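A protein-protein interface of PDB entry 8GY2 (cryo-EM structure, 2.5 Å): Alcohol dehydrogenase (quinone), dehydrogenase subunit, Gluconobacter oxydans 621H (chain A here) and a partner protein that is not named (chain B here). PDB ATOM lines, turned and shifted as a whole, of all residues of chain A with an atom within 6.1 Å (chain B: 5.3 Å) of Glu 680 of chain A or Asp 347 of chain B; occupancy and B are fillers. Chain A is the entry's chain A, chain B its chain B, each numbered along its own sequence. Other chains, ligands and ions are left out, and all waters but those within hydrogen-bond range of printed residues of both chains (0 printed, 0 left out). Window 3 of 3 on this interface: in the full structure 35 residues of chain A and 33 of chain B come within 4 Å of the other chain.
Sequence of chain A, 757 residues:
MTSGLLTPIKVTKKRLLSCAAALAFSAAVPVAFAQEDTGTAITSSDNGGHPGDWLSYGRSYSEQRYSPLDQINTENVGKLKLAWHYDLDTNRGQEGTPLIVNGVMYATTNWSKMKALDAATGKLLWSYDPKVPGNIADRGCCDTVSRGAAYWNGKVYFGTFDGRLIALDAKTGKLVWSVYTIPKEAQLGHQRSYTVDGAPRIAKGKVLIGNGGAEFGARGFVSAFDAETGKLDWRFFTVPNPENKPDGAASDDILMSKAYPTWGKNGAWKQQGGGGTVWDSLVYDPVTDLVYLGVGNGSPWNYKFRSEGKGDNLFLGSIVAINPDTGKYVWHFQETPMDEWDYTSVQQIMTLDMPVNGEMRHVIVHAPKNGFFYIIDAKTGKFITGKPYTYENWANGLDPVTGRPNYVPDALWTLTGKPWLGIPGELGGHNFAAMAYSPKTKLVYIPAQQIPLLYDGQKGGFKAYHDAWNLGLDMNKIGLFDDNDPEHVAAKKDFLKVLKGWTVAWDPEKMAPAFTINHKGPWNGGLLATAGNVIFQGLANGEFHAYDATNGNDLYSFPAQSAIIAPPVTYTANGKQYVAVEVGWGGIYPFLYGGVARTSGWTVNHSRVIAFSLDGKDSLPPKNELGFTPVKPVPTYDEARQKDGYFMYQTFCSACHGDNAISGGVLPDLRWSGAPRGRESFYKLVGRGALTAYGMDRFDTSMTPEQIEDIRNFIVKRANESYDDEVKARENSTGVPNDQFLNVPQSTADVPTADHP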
ATOM      1  N   GLY A 678       0.555  24.206   4.874  1.00  0.00           N
ATOM      2  CA  GLY A 678       0.066  22.927   5.357  1.00  0.00           C
ATOM      3  C   GLY A 678      -1.369  23.041   5.808  1.00  0.00           C
ATOM      4  O   GLY A 678      -1.842  24.123   6.169  1.00  0.00           O
ATOM      5  N   ARG A 679      -2.073  21.909   5.782  1.00  0.00           N
ATOM      6  CA  ARG A 679      -3.479  21.898   6.177  1.00  0.00           C
ATOM      7  C   ARG A 679      -3.635  22.160   7.671  1.00  0.00           C
ATOM      8  O   ARG A 679      -4.478  22.966   8.086  1.00  0.00           O
ATOM      9  CB  ARG A 679      -4.117  20.564   5.793  1.00  0.00           C
ATOM     10  CG  ARG A 679      -5.459  20.298   6.449  1.00  0.00           C
ATOM     11  CD  ARG A 679      -5.882  18.851   6.268  1.00  0.00           C
ATOM     12  NE  ARG A 679      -6.981  18.712   5.318  1.00  0.00           N
ATOM     13  CZ  ARG A 679      -8.264  18.778   5.643  1.00  0.00           C
ATOM     14  NH1 ARG A 679      -8.654  18.988   6.889  1.00  0.00           N
ATOM     15  NH2 ARG A 679      -9.182  18.630   4.691  1.00  0.00           N
ATOM     16  N   GLU A 680      -2.822  21.493   8.492  1.00  0.00           N
ATOM     17  CA  GLU A 680      -2.981  21.593   9.939  1.00  0.00           C
ATOM     18  C   GLU A 680      -2.682  23.000  10.438  1.00  0.00           C
ATOM     19  O   GLU A 680      -3.439  23.555  11.242  1.00  0.00           O
ATOM     20  CB  GLU A 680      -2.083  20.575  10.640  1.00  0.00           C
ATOM     21  CG  GLU A 680      -1.969  20.797  12.138  1.00  0.00           C
ATOM     22  CD  GLU A 680      -1.103  19.761  12.822  1.00  0.00           C
ATOM     23  OE1 GLU A 680      -0.330  19.074  12.124  1.00  0.00           O
ATOM     24  OE2 GLU A 680      -1.197  19.636  14.060  1.00  0.00           O
ATOM     25  N   SER A 681      -1.574  23.590   9.984  1.00  0.00           N
ATOM     26  CA  SER A 681      -1.218  24.933  10.431  1.00  0.00           C
ATOM     27  C   SER A 681      -2.260  25.952   9.992  1.00  0.00           C
ATOM     28  O   SER A 681      -2.645  26.837  10.768  1.00  0.00           O
ATOM     29  CB  SER A 681       0.163  25.314   9.901  1.00  0.00           C
ATOM     30  OG  SER A 681       0.118  25.593   8.514  1.00  0.00           O
ATOM     31  N   PHE A 682      -2.738  25.835   8.752  1.00  0.00           N
ATOM     32  CA  PHE A 682      -3.757  26.757   8.267  1.00  0.00           C
ATOM     33  C   PHE A 682      -5.040  26.637   9.075  1.00  0.00           C
ATOM     34  O   PHE A 682      -5.657  27.650   9.422  1.00  0.00           O
ATOM     35  CB  PHE A 682      -4.033  26.511   6.787  1.00  0.00           C
ATOM     36  CG  PHE A 682      -4.815  27.609   6.131  1.00  0.00           C
ATOM     37  CD1 PHE A 682      -4.221  28.823   5.838  1.00  0.00           C
ATOM     38  CD2 PHE A 682      -6.150  27.432   5.817  1.00  0.00           C
ATOM     39  CE1 PHE A 682      -4.940  29.833   5.237  1.00  0.00           C
ATOM     40  CE2 PHE A 682      -6.873  28.439   5.215  1.00  0.00           C
ATOM     41  CZ  PHE A 682      -6.267  29.640   4.926  1.00  0.00           C
ATOM     42  N   TYR A 683      -5.466  25.408   9.382  1.00  0.00           N
ATOM     43  CA  TYR A 683      -6.673  25.253  10.188  1.00  0.00           C
ATOM     44  C   TYR A 683      -6.476  25.797  11.597  1.00  0.00           C
ATOM     45  O   TYR A 683      -7.360  26.474  12.132  1.00  0.00           O
ATOM     46  CB  TYR A 683      -7.107  23.791  10.248  1.00  0.00           C
ATOM     47  CG  TYR A 683      -8.377  23.611  11.046  1.00  0.00           C
ATOM     48  CD1 TYR A 683      -9.604  24.005  10.530  1.00  0.00           C
ATOM     49  CD2 TYR A 683      -8.348  23.078  12.327  1.00  0.00           C
ATOM     50  CE1 TYR A 683     -10.766  23.856  11.258  1.00  0.00           C
ATOM     51  CE2 TYR A 683      -9.506  22.925  13.064  1.00  0.00           C
ATOM     52  CZ  TYR A 683     -10.712  23.315  12.524  1.00  0.00           C
ATOM     53  OH  TYR A 683     -11.868  23.165  13.253  1.00  0.00           O
ATOM     54  N   LYS A 684      -5.329  25.513  12.216  1.00  0.00           N
ATOM     55  CA  LYS A 684      -5.087  25.993  13.571  1.00  0.00           C
ATOM     56  C   LYS A 684      -4.961  27.507  13.629  1.00  0.00           C
ATOM     57  O   LYS A 684      -5.178  28.093  14.695  1.00  0.00           O
ATOM     58  CB  LYS A 684      -3.834  25.337  14.150  1.00  0.00           C
ATOM     59  CG  LYS A 684      -3.956  23.832  14.321  1.00  0.00           C
ATOM     60  CD  LYS A 684      -3.096  23.325  15.462  1.00  0.00           C
ATOM     61  CE  LYS A 684      -3.615  22.001  15.991  1.00  0.00           C
ATOM     62  NZ  LYS A 684      -2.521  21.012  16.189  1.00  0.00           N
ATOM     63  N   LEU A 685      -4.612  28.153  12.519  1.00  0.00           N
ATOM     64  CA  LEU A 685      -4.604  29.610  12.498  1.00  0.00           C
ATOM     65  C   LEU A 685      -5.979  30.197  12.204  1.00  0.00           C
ATOM     66  O   LEU A 685      -6.373  31.183  12.834  1.00  0.00           O
ATOM     67  CB  LEU A 685      -3.594  30.119  11.470  1.00  0.00           C
ATOM     68  CG  LEU A 685      -2.351  30.763  12.077  1.00  0.00           C
ATOM     69  CD1 LEU A 685      -1.109  30.058  11.576  1.00  0.00           C
ATOM     70  CD2 LEU A 685      -2.307  32.246  11.753  1.00  0.00           C
ATOM     71  N   GLU A 709      -9.953  24.461   4.123  1.00  0.00           N
ATOM     72  CA  GLU A 709      -8.989  23.851   3.212  1.00  0.00           C
ATOM     73  C   GLU A 709      -9.152  24.387   1.794  1.00  0.00           C
ATOM     74  O   GLU A 709      -8.164  24.569   1.072  1.00  0.00           O
ATOM     75  CB  GLU A 709      -9.140  22.331   3.235  1.00  0.00           C
ATOM     76  CG  GLU A 709      -8.134  21.588   2.371  1.00  0.00           C
ATOM     77  CD  GLU A 709      -6.701  21.821   2.805  1.00  0.00           C
ATOM     78  OE1 GLU A 709      -6.477  22.113   3.997  1.00  0.00           O
ATOM     79  OE2 GLU A 709      -5.797  21.710   1.952  1.00  0.00           O
ATOM     80  N   ARG A 712      -7.461  27.608   1.703  1.00  0.00           N
ATOM     81  CA  ARG A 712      -6.016  27.407   1.660  1.00  0.00           C
ATOM     82  C   ARG A 712      -5.546  27.073   0.251  1.00  0.00           C
ATOM     83  O   ARG A 712      -4.528  27.601  -0.217  1.00  0.00           O
ATOM     84  CB  ARG A 712      -5.611  26.296   2.625  1.00  0.00           C
ATOM     85  CG  ARG A 712      -4.113  26.068   2.708  1.00  0.00           C
ATOM     86  CD  ARG A 712      -3.786  24.848   3.546  1.00  0.00           C
ATOM     87  NE  ARG A 712      -3.932  23.610   2.791  1.00  0.00           N
ATOM     88  CZ  ARG A 712      -3.037  23.147   1.930  1.00  0.00           C
ATOM     89  NH1 ARG A 712      -1.911  23.796   1.688  1.00  0.00           N
ATOM     90  NH2 ARG A 712      -3.278  22.003   1.298  1.00  0.00           N
ATOM     91  N   THR B 320       3.664  12.149  16.741  1.00  0.00           N
ATOM     92  CA  THR B 320       2.516  12.723  16.047  1.00  0.00           C
ATOM     93  C   THR B 320       1.275  11.859  16.228  1.00  0.00           C
ATOM     94  O   THR B 320       0.176  12.379  16.449  1.00  0.00           O
ATOM     95  CB  THR B 320       2.833  12.903  14.563  1.00  0.00           C
ATOM     96  OG1 THR B 320       4.134  13.485  14.420  1.00  0.00           O
ATOM     97  CG2 THR B 320       1.807  13.813  13.909  1.00  0.00           C
ATOM     98  N   LEU B 323      -0.015  12.343  19.794  1.00  0.00           N
ATOM     99  CA  LEU B 323      -0.725  13.606  19.963  1.00  0.00           C
ATOM    100  C   LEU B 323      -2.052  13.613  19.213  1.00  0.00           C
ATOM    101  O   LEU B 323      -3.006  14.262  19.655  1.00  0.00           O
ATOM    102  CB  LEU B 323       0.156  14.768  19.509  1.00  0.00           C
ATOM    103  CG  LEU B 323       1.312  15.097  20.456  1.00  0.00           C
ATOM    104  CD1 LEU B 323       2.299  16.041  19.797  1.00  0.00           C
ATOM    105  CD2 LEU B 323       0.788  15.688  21.753  1.00  0.00           C
ATOM    106  N   ALA B 341       0.161  22.778  21.426  1.00  0.00           N
ATOM    107  CA  ALA B 341      -0.031  22.214  20.095  1.00  0.00           C
ATOM    108  C   ALA B 341      -0.751  23.163  19.147  1.00  0.00           C
ATOM    109  O   ALA B 341      -0.686  22.966  17.930  1.00  0.00           O
ATOM    110  CB  ALA B 341      -0.801  20.896  20.187  1.00  0.00           C
ATOM    111  N   HIS B 344       2.417  25.232  17.721  1.00  0.00           N
ATOM    112  CA  HIS B 344       3.563  24.483  17.225  1.00  0.00           C
ATOM    113  C   HIS B 344       3.176  23.180  16.537  1.00  0.00           C
ATOM    114  O   HIS B 344       4.061  22.385  16.207  1.00  0.00           O
ATOM    115  CB  HIS B 344       4.539  24.204  18.370  1.00  0.00           C
ATOM    116  CG  HIS B 344       5.197  25.433  18.912  1.00  0.00           C
ATOM    117  ND1 HIS B 344       6.168  26.123  18.221  1.00  0.00           N
ATOM    118  CD2 HIS B 344       5.023  26.098  20.079  1.00  0.00           C
ATOM    119  CE1 HIS B 344       6.564  27.159  18.937  1.00  0.00           C
ATOM    120  NE2 HIS B 344       5.885  27.167  20.070  1.00  0.00           N
ATOM    121  N   MET B 345       1.880  22.942  16.321  1.00  0.00           N
ATOM    122  CA  MET B 345       1.381  21.788  15.575  1.00  0.00           C
ATOM    123  C   MET B 345       1.664  20.466  16.279  1.00  0.00           C
ATOM    124  O   MET B 345       2.485  20.399  17.198  1.00  0.00           O
ATOM    125  CB  MET B 345       1.967  21.767  14.159  1.00  0.00           C
ATOM    126  CG  MET B 345       1.692  23.029  13.367  1.00  0.00           C
ATOM    127  SD  MET B 345      -0.007  23.581  13.576  1.00  0.00           S
ATOM    128  CE  MET B 345       0.239  25.326  13.884  1.00  0.00           C
ATOM    129  N   ASN B 346       0.968  19.409  15.860  1.00  0.00           N
ATOM    130  CA  ASN B 346       1.136  18.091  16.456  1.00  0.00           C
ATOM    131  C   ASN B 346       2.414  17.394  16.014  1.00  0.00           C
ATOM    132  O   ASN B 346       2.817  16.417  16.654  1.00  0.00           O
ATOM    133  CB  ASN B 346      -0.068  17.209  16.121  1.00  0.00           C
ATOM    134  CG  ASN B 346      -1.279  17.532  16.969  1.00  0.00           C
ATOM    135  OD1 ASN B 346      -1.377  18.617  17.542  1.00  0.00           O
ATOM    136  ND2 ASN B 346      -2.211  16.593  17.050  1.00  0.00           N
ATOM    137  N   ASP B 347       3.055  17.856  14.944  1.00  0.00           N
ATOM    138  CA  ASP B 347       4.322  17.299  14.496  1.00  0.00           C
ATOM    139  C   ASP B 347       5.514  18.149  14.914  1.00  0.00           C
ATOM    140  O   ASP B 347       6.642  17.859  14.505  1.00  0.00           O
ATOM    141  CB  ASP B 347       4.311  17.109  12.977  1.00  0.00           C
ATOM    142  CG  ASP B 347       3.831  18.341  12.235  1.00  0.00           C
ATOM    143  OD1 ASP B 347       3.860  19.444  12.816  1.00  0.00           O
ATOM    144  OD2 ASP B 347       3.424  18.205  11.063  1.00  0.00           O
ATOM    145  N   GLY B 348       5.290  19.190  15.714  1.00  0.00           N
ATOM    146  CA  GLY B 348       6.382  20.013  16.191  1.00  0.00           C
ATOM    147  C   GLY B 348       7.031  20.881  15.142  1.00  0.00           C
ATOM    148  O   GLY B 348       8.145  21.362  15.357  1.00  0.00           O
ATOM    149  N   THR B 349       6.366  21.100  14.008  1.00  0.00           N
ATOM    150  CA  THR B 349       6.938  21.881  12.921  1.00  0.00           C
ATOM    151  C   THR B 349       6.551  23.352  12.961  1.00  0.00           C
ATOM    152  O   THR B 349       7.222  24.167  12.318  1.00  0.00           O
ATOM    153  CB  THR B 349       6.519  21.294  11.569  1.00  0.00           C
ATOM    154  OG1 THR B 349       5.095  21.145  11.533  1.00  0.00           O
ATOM    155  CG2 THR B 349       7.169  19.938  11.355  1.00  0.00           C
ATOM    156  N   GLY B 350       5.498  23.710  13.690  1.00  0.00           N
ATOM    157  CA  GLY B 350       5.105  25.100  13.784  1.00  0.00           C
ATOM    158  C   GLY B 350       4.628  25.663  12.454  1.00  0.00           C
ATOM    159  O   GLY B 350       4.196  24.944  11.549  1.00  0.00           O
ATOM    160  N   ALA B 359      10.556  20.401  16.536  1.00  0.00           N
ATOM    161  CA  ALA B 359      11.181  19.163  16.093  1.00  0.00           C
ATOM    162  C   ALA B 359      12.462  19.499  15.340  1.00  0.00           C
ATOM    163  O   ALA B 359      12.418  20.143  14.286  1.00  0.00           O
ATOM    164  CB  ALA B 359      10.230  18.365  15.206  1.00  0.00           C
ATOM    165  N   TRP B 417       9.307  13.675  18.506  1.00  0.00           N
ATOM    166  CA  TRP B 417       9.520  13.890  17.072  1.00  0.00           C
ATOM    167  C   TRP B 417      10.963  13.606  16.664  1.00  0.00           C
ATOM    168  O   TRP B 417      11.547  14.316  15.844  1.00  0.00           O
ATOM    169  CB  TRP B 417       9.117  15.306  16.652  1.00  0.00           C
ATOM    170  CG  TRP B 417       7.800  15.759  17.185  1.00  0.00           C
ATOM    171  CD1 TRP B 417       6.567  15.326  16.801  1.00  0.00           C
ATOM    172  CD2 TRP B 417       7.581  16.757  18.189  1.00  0.00           C
ATOM    173  NE1 TRP B 417       5.593  15.984  17.511  1.00  0.00           N
ATOM    174  CE2 TRP B 417       6.190  16.869  18.368  1.00  0.00           C
ATOM    175  CE3 TRP B 417       8.427  17.563  18.956  1.00  0.00           C
ATOM    176  CZ2 TRP B 417       5.626  17.753  19.283  1.00  0.00           C
ATOM    177  CZ3 TRP B 417       7.865  18.440  19.862  1.00  0.00           C
ATOM    178  CH2 TRP B 417       6.478  18.528  20.018  1.00  0.00           C
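Printed residues of chain B within 4 Å of Lys 684 of chain A: Ala 341 (3.2 Å), Met 345 (3.6 Å) and Asn 346 (3.0 Å).
Of the printed residues of chain A, Asn 346 of chain B touches Glu 680 (2.8 Å) and Lys 684 (3.0 Å).
Printed residues of chain A within 4 Å of Asp 347 of chain B: Glu 680.
Gly 350 of chain B touches none of the printed residues of chain A.
The nearest printed residue of chain B that does not touch Glu 680 of chain A is Ala 341 of chain B (5.1 Å).
The nearest printed residue of chain A that does not touch Asp 347 of chain B is Lys 684 of chain A (6.5 Å).
NZ of Lys 684 of chain A lies within hydrogen-bond range of O of Ala 341 of chain B (3.2 Å).
NZ of Lys 684 of chain A sits at hydrogen-bond distance from OD1 of Asn 346 of chain B, 3.0 Å away.
The backbone NH of Asn 346 of chain B sits at hydrogen-bond distance from the side-chain carboxylate of Glu 680 of chain A, 2.8 Å away.
The backbone carbonyl oxygen (O) of Gly 678 of chain A is in hydrogen-bond range of the side-chain hydroxyl (OG) of Ser 681 of chain A, at 3.4 Å.
The side-chain carboxylate of Asp 347 of chain B sits at hydrogen-bond distance from the side-chain hydroxyl of Thr 349 of chain B (2.5 Å).
The side-chain amino group (NZ) of Lys 684 of chain A lies within salt-bridge range of the side-chain carboxylate (OE2) of Glu 680 of chain A.
The backbone carbonyl oxygen of Asn 346 of chain B is in hydrogen-bond range of the indole nitrogen of Trp 417 of chain B.
Hydrophobic or aromatic side chains of chain B within 4 Å of the printed part of chain A: Met 345.
Along chain B the printed residues that touch a printed residue of chain A span positions 341 to 347.
Printed residues of chain A that touch a printed residue of chain B: Glu 680, Ser 681 and Lys 684.
Among the printed residues, no Asp or Glu carboxylate lies within 4 Å of a Lys or Arg side-chain nitrogen of the other chain.
CA of Met 345 of chain B touches OE2 of Glu 680 of chain A, at 3.7 Å.
Glu 680 of chain A touches Asp 347 of chain B.
Met 345 of chain B touches Ser 681 of chain A (SD to CA, 3.6 Å).
Lys 684 of chain A touches Met 345 of chain B (CD to SD, 3.6 Å).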
